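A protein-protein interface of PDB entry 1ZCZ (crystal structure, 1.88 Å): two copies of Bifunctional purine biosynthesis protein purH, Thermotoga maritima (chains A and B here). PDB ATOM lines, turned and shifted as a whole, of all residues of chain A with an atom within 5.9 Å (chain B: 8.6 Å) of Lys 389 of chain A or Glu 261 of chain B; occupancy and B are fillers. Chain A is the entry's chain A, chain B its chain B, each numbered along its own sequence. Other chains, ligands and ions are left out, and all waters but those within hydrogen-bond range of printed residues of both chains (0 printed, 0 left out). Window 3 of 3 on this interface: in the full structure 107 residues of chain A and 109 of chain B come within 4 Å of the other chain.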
ATOM      1  N   SER A 387     -25.925   6.452 -25.314  1.00  0.00           N
ATOM      2  CA  SER A 387     -26.423   5.107 -25.641  1.00  0.00           C
ATOM      3  C   SER A 387     -27.845   4.976 -25.122  1.00  0.00           C
ATOM      4  O   SER A 387     -28.231   5.662 -24.159  1.00  0.00           O
ATOM      5  CB  SER A 387     -25.542   4.020 -25.009  1.00  0.00           C
ATOM      6  OG  SER A 387     -25.974   3.736 -23.690  1.00  0.00           O
ATOM      7  N   ARG A 388     -28.618   4.086 -25.742  1.00  0.00           N
ATOM      8  CA  ARG A 388     -30.036   4.009 -25.463  1.00  0.00           C
ATOM      9  C   ARG A 388     -30.243   3.288 -24.136  1.00  0.00           C
ATOM     10  O   ARG A 388     -31.121   3.659 -23.366  1.00  0.00           O
ATOM     11  CB  ARG A 388     -30.812   3.346 -26.613  1.00  0.00           C
ATOM     12  CG  ARG A 388     -32.328   3.185 -26.300  1.00  0.00           C
ATOM     13  CD  ARG A 388     -33.274   3.661 -27.383  1.00  0.00           C
ATOM     14  NE  ARG A 388     -32.729   4.769 -28.161  1.00  0.00           N
ATOM     15  CZ  ARG A 388     -33.041   6.059 -28.000  1.00  0.00           C
ATOM     16  NH1 ARG A 388     -33.937   6.456 -27.099  1.00  0.00           N
ATOM     17  NH2 ARG A 388     -32.461   6.974 -28.777  1.00  0.00           N
ATOM     18  N   LYS A 389     -29.391   2.293 -23.874  1.00  0.00           N
ATOM     19  CA  LYS A 389     -29.400   1.569 -22.624  1.00  0.00           C
ATOM     20  C   LYS A 389     -29.252   2.532 -21.456  1.00  0.00           C
ATOM     21  O   LYS A 389     -29.943   2.398 -20.461  1.00  0.00           O
ATOM     22  CB  LYS A 389     -28.244   0.590 -22.609  1.00  0.00           C
ATOM     23  CG  LYS A 389     -28.142  -0.219 -21.358  1.00  0.00           C
ATOM     24  CD  LYS A 389     -26.838  -0.948 -21.313  1.00  0.00           C
ATOM     25  CE  LYS A 389     -26.512  -1.374 -19.882  1.00  0.00           C
ATOM     26  NZ  LYS A 389     -25.268  -2.219 -19.847  1.00  0.00           N
ATOM     27  N   ARG A 390     -28.348   3.498 -21.580  1.00  0.00           N
ATOM     28  CA  ARG A 390     -28.150   4.473 -20.505  1.00  0.00           C
ATOM     29  C   ARG A 390     -29.328   5.362 -20.282  1.00  0.00           C
ATOM     30  O   ARG A 390     -29.714   5.601 -19.138  1.00  0.00           O
ATOM     31  CB  ARG A 390     -26.950   5.325 -20.761  1.00  0.00           C
ATOM     32  CG  ARG A 390     -25.834   4.759 -20.044  1.00  0.00           C
ATOM     33  CD  ARG A 390     -24.529   5.392 -20.476  1.00  0.00           C
ATOM     34  NE  ARG A 390     -24.417   6.762 -19.995  1.00  0.00           N
ATOM     35  CZ  ARG A 390     -23.323   7.496 -20.113  1.00  0.00           C
ATOM     36  NH1 ARG A 390     -22.238   6.985 -20.698  1.00  0.00           N
ATOM     37  NH2 ARG A 390     -23.287   8.720 -19.618  1.00  0.00           N
ATOM     38  N   ALA A 391     -29.903   5.849 -21.367  1.00  0.00           N
ATOM     39  CA  ALA A 391     -31.149   6.587 -21.284  1.00  0.00           C
ATOM     40  C   ALA A 391     -32.251   5.835 -20.515  1.00  0.00           C
ATOM     41  O   ALA A 391     -32.883   6.395 -19.615  1.00  0.00           O
ATOM     42  CB  ALA A 391     -31.621   6.992 -22.689  1.00  0.00           C
ATOM     43  N   ALA A 392     -32.472   4.573 -20.867  1.00  0.00           N
ATOM     44  CA  ALA A 392     -33.465   3.748 -20.210  1.00  0.00           C
ATOM     45  C   ALA A 392     -33.145   3.567 -18.728  1.00  0.00           C
ATOM     46  O   ALA A 392     -34.034   3.547 -17.905  1.00  0.00           O
ATOM     47  CB  ALA A 392     -33.527   2.339 -20.904  1.00  0.00           C
ATOM     48  N   TRP A 393     -31.866   3.367 -18.422  1.00  0.00           N
ATOM     49  CA  TRP A 393     -31.418   3.184 -17.049  1.00  0.00           C
ATOM     50  C   TRP A 393     -31.721   4.433 -16.209  1.00  0.00           C
ATOM     51  O   TRP A 393     -32.369   4.327 -15.168  1.00  0.00           O
ATOM     52  CB  TRP A 393     -29.927   2.801 -17.019  1.00  0.00           C
ATOM     53  CG  TRP A 393     -29.300   2.957 -15.658  1.00  0.00           C
ATOM     54  CD1 TRP A 393     -29.485   2.182 -14.567  1.00  0.00           C
ATOM     55  CD2 TRP A 393     -28.418   4.009 -15.266  1.00  0.00           C
ATOM     56  NE1 TRP A 393     -28.762   2.683 -13.503  1.00  0.00           N
ATOM     57  CE2 TRP A 393     -28.102   3.810 -13.918  1.00  0.00           C
ATOM     58  CE3 TRP A 393     -27.860   5.102 -15.944  1.00  0.00           C
ATOM     59  CZ2 TRP A 393     -27.246   4.659 -13.220  1.00  0.00           C
ATOM     60  CZ3 TRP A 393     -27.003   5.943 -15.252  1.00  0.00           C
ATOM     61  CH2 TRP A 393     -26.709   5.713 -13.903  1.00  0.00           C
ATOM     62  N   ILE A 394     -31.307   5.606 -16.679  1.00  0.00           N
ATOM     63  CA  ILE A 394     -31.631   6.864 -15.955  1.00  0.00           C
ATOM     64  C   ILE A 394     -33.132   7.073 -15.778  1.00  0.00           C
ATOM     65  O   ILE A 394     -33.576   7.456 -14.700  1.00  0.00           O
ATOM     66  CB  ILE A 394     -30.981   8.102 -16.613  1.00  0.00           C
ATOM     67  CG1 ILE A 394     -29.452   7.974 -16.564  1.00  0.00           C
ATOM     68  CG2 ILE A 394     -31.398   9.383 -15.907  1.00  0.00           C
ATOM     69  CD1 ILE A 394     -28.765   8.950 -17.403  1.00  0.00           C
ATOM     70  N   ASP A 418     -31.748  -5.432 -24.536  1.00  0.00           N
ATOM     71  CA  ASP A 418     -31.358  -4.996 -23.187  1.00  0.00           C
ATOM     72  C   ASP A 418     -32.059  -3.726 -22.694  1.00  0.00           C
ATOM     73  O   ASP A 418     -32.488  -3.663 -21.533  1.00  0.00           O
ATOM     74  CB  ASP A 418     -29.818  -4.920 -23.017  1.00  0.00           C
ATOM     75  CG  ASP A 418     -29.157  -3.843 -23.864  1.00  0.00           C
ATOM     76  OD1 ASP A 418     -29.826  -3.172 -24.675  1.00  0.00           O
ATOM     77  OD2 ASP A 418     -27.932  -3.654 -23.710  1.00  0.00           O
ATOM     78  N   SER A 419     -32.233  -2.740 -23.572  1.00  0.00           N
ATOM     79  CA  SER A 419     -32.930  -1.482 -23.211  1.00  0.00           C
ATOM     80  C   SER A 419     -34.387  -1.722 -22.845  1.00  0.00           C
ATOM     81  O   SER A 419     -34.914  -1.143 -21.890  1.00  0.00           O
ATOM     82  CB  SER A 419     -32.841  -0.458 -24.348  1.00  0.00           C
ATOM     83  OG  SER A 419     -31.527   0.038 -24.460  1.00  0.00           O
ATOM     84  N   ILE A 422     -34.670  -3.475 -19.320  1.00  0.00           N
ATOM     85  CA  ILE A 422     -34.562  -2.541 -18.193  1.00  0.00           C
ATOM     86  C   ILE A 422     -35.919  -1.924 -17.862  1.00  0.00           C
ATOM     87  O   ILE A 422     -36.310  -1.854 -16.710  1.00  0.00           O
ATOM     88  CB  ILE A 422     -33.513  -1.433 -18.510  1.00  0.00           C
ATOM     89  CG1 ILE A 422     -32.093  -2.011 -18.458  1.00  0.00           C
ATOM     90  CG2 ILE A 422     -33.609  -0.264 -17.558  1.00  0.00           C
ATOM     91  CD1 ILE A 422     -31.113  -1.221 -19.291  1.00  0.00           C
ATOM     92  N   LYS B 235     -20.678  11.258 -29.449  1.00  0.00           N
ATOM     93  CA  LYS B 235     -21.894  10.523 -29.765  1.00  0.00           C
ATOM     94  C   LYS B 235     -23.052  11.438 -29.401  1.00  0.00           C
ATOM     95  O   LYS B 235     -23.047  12.014 -28.316  1.00  0.00           O
ATOM     96  CB  LYS B 235     -21.895   9.250 -28.914  1.00  0.00           C
ATOM     97  CG  LYS B 235     -22.751   8.188 -29.395  1.00  0.00           C
ATOM     98  CD  LYS B 235     -22.181   7.528 -30.610  1.00  0.00           C
ATOM     99  CE  LYS B 235     -22.942   6.284 -30.855  1.00  0.00           C
ATOM    100  NZ  LYS B 235     -22.837   5.365 -29.684  1.00  0.00           N
ATOM    101  N   CYS B 240     -18.121  11.433 -25.614  1.00  0.00           N
ATOM    102  CA  CYS B 240     -18.171  10.282 -24.729  1.00  0.00           C
ATOM    103  C   CYS B 240     -16.779   9.862 -24.211  1.00  0.00           C
ATOM    104  O   CYS B 240     -16.663   9.166 -23.175  1.00  0.00           O
ATOM    105  CB  CYS B 240     -18.911   9.133 -25.403  1.00  0.00           C
ATOM    106  SG  CYS B 240     -18.137   8.468 -26.844  1.00  0.00           S
ATOM    107  N   ILE B 256     -11.292   6.144 -27.447  1.00  0.00           N
ATOM    108  CA  ILE B 256     -12.318   5.187 -27.886  1.00  0.00           C
ATOM    109  C   ILE B 256     -12.791   4.285 -26.730  1.00  0.00           C
ATOM    110  O   ILE B 256     -13.985   4.040 -26.542  1.00  0.00           O
ATOM    111  CB  ILE B 256     -11.765   4.340 -29.087  1.00  0.00           C
ATOM    112  CG1 ILE B 256     -11.787   5.185 -30.372  1.00  0.00           C
ATOM    113  CG2 ILE B 256     -12.526   3.009 -29.256  1.00  0.00           C
ATOM    114  CD1 ILE B 256     -10.949   4.566 -31.536  1.00  0.00           C
ATOM    115  N   GLU B 257     -11.833   3.764 -25.973  1.00  0.00           N
ATOM    116  CA  GLU B 257     -12.132   2.839 -24.897  1.00  0.00           C
ATOM    117  C   GLU B 257     -12.616   3.502 -23.582  1.00  0.00           C
ATOM    118  O   GLU B 257     -13.106   2.809 -22.711  1.00  0.00           O
ATOM    119  CB  GLU B 257     -10.906   1.980 -24.631  1.00  0.00           C
ATOM    120  CG  GLU B 257     -10.649   0.992 -25.719  1.00  0.00           C
ATOM    121  CD  GLU B 257      -9.490   0.048 -25.385  1.00  0.00           C
ATOM    122  OE1 GLU B 257      -8.749   0.313 -24.398  1.00  0.00           O
ATOM    123  OE2 GLU B 257      -9.327  -0.944 -26.126  1.00  0.00           O
ATOM    124  N   ALA B 258     -12.521   4.830 -23.469  1.00  0.00           N
ATOM    125  CA  ALA B 258     -12.898   5.537 -22.248  1.00  0.00           C
ATOM    126  C   ALA B 258     -14.352   5.236 -21.854  1.00  0.00           C
ATOM    127  O   ALA B 258     -14.640   4.900 -20.687  1.00  0.00           O
ATOM    128  CB  ALA B 258     -12.671   7.006 -22.401  1.00  0.00           C
ATOM    129  N   ASP B 259     -15.263   5.386 -22.819  1.00  0.00           N
ATOM    130  CA  ASP B 259     -16.613   4.890 -22.685  1.00  0.00           C
ATOM    131  C   ASP B 259     -16.846   3.900 -23.828  1.00  0.00           C
ATOM    132  O   ASP B 259     -17.511   4.205 -24.834  1.00  0.00           O
ATOM    133  CB  ASP B 259     -17.616   6.029 -22.715  1.00  0.00           C
ATOM    134  CG  ASP B 259     -19.044   5.551 -22.537  1.00  0.00           C
ATOM    135  OD1 ASP B 259     -19.245   4.333 -22.345  1.00  0.00           O
ATOM    136  OD2 ASP B 259     -19.961   6.401 -22.570  1.00  0.00           O
ATOM    137  N   ASP B 260     -16.315   2.702 -23.640  1.00  0.00           N
ATOM    138  CA  ASP B 260     -16.236   1.694 -24.707  1.00  0.00           C
ATOM    139  C   ASP B 260     -17.588   1.269 -25.269  1.00  0.00           C
ATOM    140  O   ASP B 260     -17.695   0.985 -26.463  1.00  0.00           O
ATOM    141  CB  ASP B 260     -15.464   0.463 -24.214  1.00  0.00           C
ATOM    142  CG  ASP B 260     -15.124  -0.513 -25.334  1.00  0.00           C
ATOM    143  OD1 ASP B 260     -14.597  -0.084 -26.381  1.00  0.00           O
ATOM    144  OD2 ASP B 260     -15.365  -1.729 -25.143  1.00  0.00           O
ATOM    145  N   GLU B 261     -18.609   1.219 -24.424  1.00  0.00           N
ATOM    146  CA  GLU B 261     -19.968   0.876 -24.864  1.00  0.00           C
ATOM    147  C   GLU B 261     -20.585   1.927 -25.798  1.00  0.00           C
ATOM    148  O   GLU B 261     -21.356   1.593 -26.710  1.00  0.00           O
ATOM    149  CB  GLU B 261     -20.882   0.710 -23.657  1.00  0.00           C
ATOM    150  CG  GLU B 261     -20.514  -0.449 -22.747  1.00  0.00           C
ATOM    151  CD  GLU B 261     -21.165  -0.354 -21.374  1.00  0.00           C
ATOM    152  OE1 GLU B 261     -21.101   0.727 -20.739  1.00  0.00           O
ATOM    153  OE2 GLU B 261     -21.732  -1.371 -20.917  1.00  0.00           O
ATOM    154  N   SER B 262     -20.256   3.196 -25.585  1.00  0.00           N
ATOM    155  CA  SER B 262     -20.827   4.289 -26.394  1.00  0.00           C
ATOM    156  C   SER B 262     -20.094   4.594 -27.696  1.00  0.00           C
ATOM    157  O   SER B 262     -20.654   5.207 -28.605  1.00  0.00           O
ATOM    158  CB  SER B 262     -20.845   5.581 -25.568  1.00  0.00           C
ATOM    159  OG  SER B 262     -21.694   5.422 -24.452  1.00  0.00           O
ATOM    160  N   SER B 263     -18.829   4.227 -27.780  1.00  0.00           N
ATOM    161  CA  SER B 263     -18.006   4.672 -28.900  1.00  0.00           C
ATOM    162  C   SER B 263     -18.261   3.927 -30.221  1.00  0.00           C
ATOM    163  O   SER B 263     -17.759   4.354 -31.275  1.00  0.00           O
ATOM    164  CB  SER B 263     -16.538   4.607 -28.507  1.00  0.00           C
ATOM    165  OG  SER B 263     -16.204   3.329 -28.071  1.00  0.00           O
ATOM    166  N   PHE B 264     -19.030   2.828 -30.188  1.00  0.00           N
ATOM    167  CA  PHE B 264     -19.412   2.150 -31.431  1.00  0.00           C
ATOM    168  C   PHE B 264     -20.277   3.115 -32.251  1.00  0.00           C
ATOM    169  O   PHE B 264     -21.276   3.622 -31.762  1.00  0.00           O
ATOM    170  CB  PHE B 264     -20.177   0.842 -31.188  1.00  0.00           C
ATOM    171  CG  PHE B 264     -20.732   0.238 -32.464  1.00  0.00           C
ATOM    172  CD1 PHE B 264     -19.946  -0.584 -33.258  1.00  0.00           C
ATOM    173  CD2 PHE B 264     -22.015   0.573 -32.914  1.00  0.00           C
ATOM    174  CE1 PHE B 264     -20.441  -1.107 -34.449  1.00  0.00           C
ATOM    175  CE2 PHE B 264     -22.516   0.058 -34.104  1.00  0.00           C
ATOM    176  CZ  PHE B 264     -21.730  -0.785 -34.872  1.00  0.00           C
ATOM    177  N   GLY B 265     -19.851   3.391 -33.480  1.00  0.00           N
ATOM    178  CA  GLY B 265     -20.593   4.274 -34.365  1.00  0.00           C
ATOM    179  C   GLY B 265     -20.326   5.730 -34.043  1.00  0.00           C
ATOM    180  O   GLY B 265     -21.061   6.604 -34.467  1.00  0.00           O
ATOM    181  N   GLY B 266     -19.276   5.983 -33.270  1.00  0.00           N
ATOM    182  CA  GLY B 266     -19.004   7.329 -32.798  1.00  0.00           C
ATOM    183  C   GLY B 266     -18.295   8.156 -33.846  1.00  0.00           C
ATOM    184  O   GLY B 266     -17.989   7.670 -34.925  1.00  0.00           O
ATOM    185  N   LYS B 284     -12.949  -0.655 -33.810  1.00  0.00           N
ATOM    186  CA  LYS B 284     -14.308  -0.223 -33.489  1.00  0.00           C
ATOM    187  C   LYS B 284     -14.792   0.416 -34.785  1.00  0.00           C
ATOM    188  O   LYS B 284     -14.066   1.228 -35.338  1.00  0.00           O
ATOM    189  CB  LYS B 284     -14.249   0.903 -32.427  1.00  0.00           C
ATOM    190  CG  LYS B 284     -15.385   0.997 -31.374  1.00  0.00           C
ATOM    191  CD  LYS B 284     -14.928   0.268 -30.105  1.00  0.00           C
ATOM    192  CE  LYS B 284     -16.065  -0.096 -29.218  1.00  0.00           C
ATOM    193  NZ  LYS B 284     -16.466   1.045 -28.389  1.00  0.00           N
ATOM    194  N   MET B 398     -20.229   6.362 -13.945  1.00  0.00           N
ATOM    195  CA  MET B 398     -19.463   5.917 -15.126  1.00  0.00           C
ATOM    196  C   MET B 398     -18.000   5.684 -14.794  1.00  0.00           C
ATOM    197  O   MET B 398     -17.397   4.743 -15.301  1.00  0.00           O
ATOM    198  CB  MET B 398     -19.590   6.936 -16.269  1.00  0.00           C
ATOM    199  CG  MET B 398     -20.983   7.058 -16.799  1.00  0.00           C
ATOM    200  SD  MET B 398     -21.629   5.472 -17.388  1.00  0.00           S
ATOM    201  CE  MET B 398     -23.237   5.527 -16.647  1.00  0.00           C
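The side-chain amino group (NZ) of Lys 389 of chain A lies within salt-bridge range of the side-chain carboxylate (OE2) of Glu 261 of chain B.
The guanidinium group (NH1) of Arg 390 of chain A is in salt-bridge range of the side-chain carboxylate (OD2) of Asp 259 of chain B.
NH1 of Arg 390 of chain A sits at hydrogen-bond distance from SD of Met 398 of chain B.
The side-chain hydroxyl (OG) of Ser 387 of chain A lies within hydrogen-bond range of the backbone NH (N) of Arg 390 of chain A (3.2 Å).
The backbone NH of Lys 389 of chain A is in hydrogen-bond range of the side-chain hydroxyl of Ser 419 of chain A, 3.2 Å away.
OD2 of Asp 259 of chain B is in hydrogen-bond range of OG of Ser 262 of chain B.
Of chain B, only Glu 261 comes within 4 Å of Lys 389 of chain A.
Of the printed residues of chain B, Arg 390 of chain A touches Asp 259 and Met 398.
Of the printed residues of chain A, Asp 259 of chain B touches Arg 390 (3.0 Å).
Of the printed residues of chain A, Glu 261 of chain B touches Lys 389.
Printed residues of chain A within 4 Å of Met 398 of chain B: Arg 390 (3.7 Å).
Printed residues of chain A that touch a printed residue of chain B: Lys 389 and Arg 390.
Of the 15 printed residues of chain B, 3 touch a printed residue of chain A.
Hydrophobic or aromatic side chains of chain B that line the printed part of chain A: Met 398.
Among the printed residues, Asp or Glu carboxylates within 4 Å of a Lys or Arg side-chain nitrogen of the other chain: Lys 389 of chain A with Glu 261 of chain B (3.8 Å) and Arg 390 of chain A with Asp 259 of chain B (3.0 Å).
No position is printed for both chains.
Of the 3 pairs that touch across the chains among the printed residues, none has its exchanged pair printed and touching as well.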
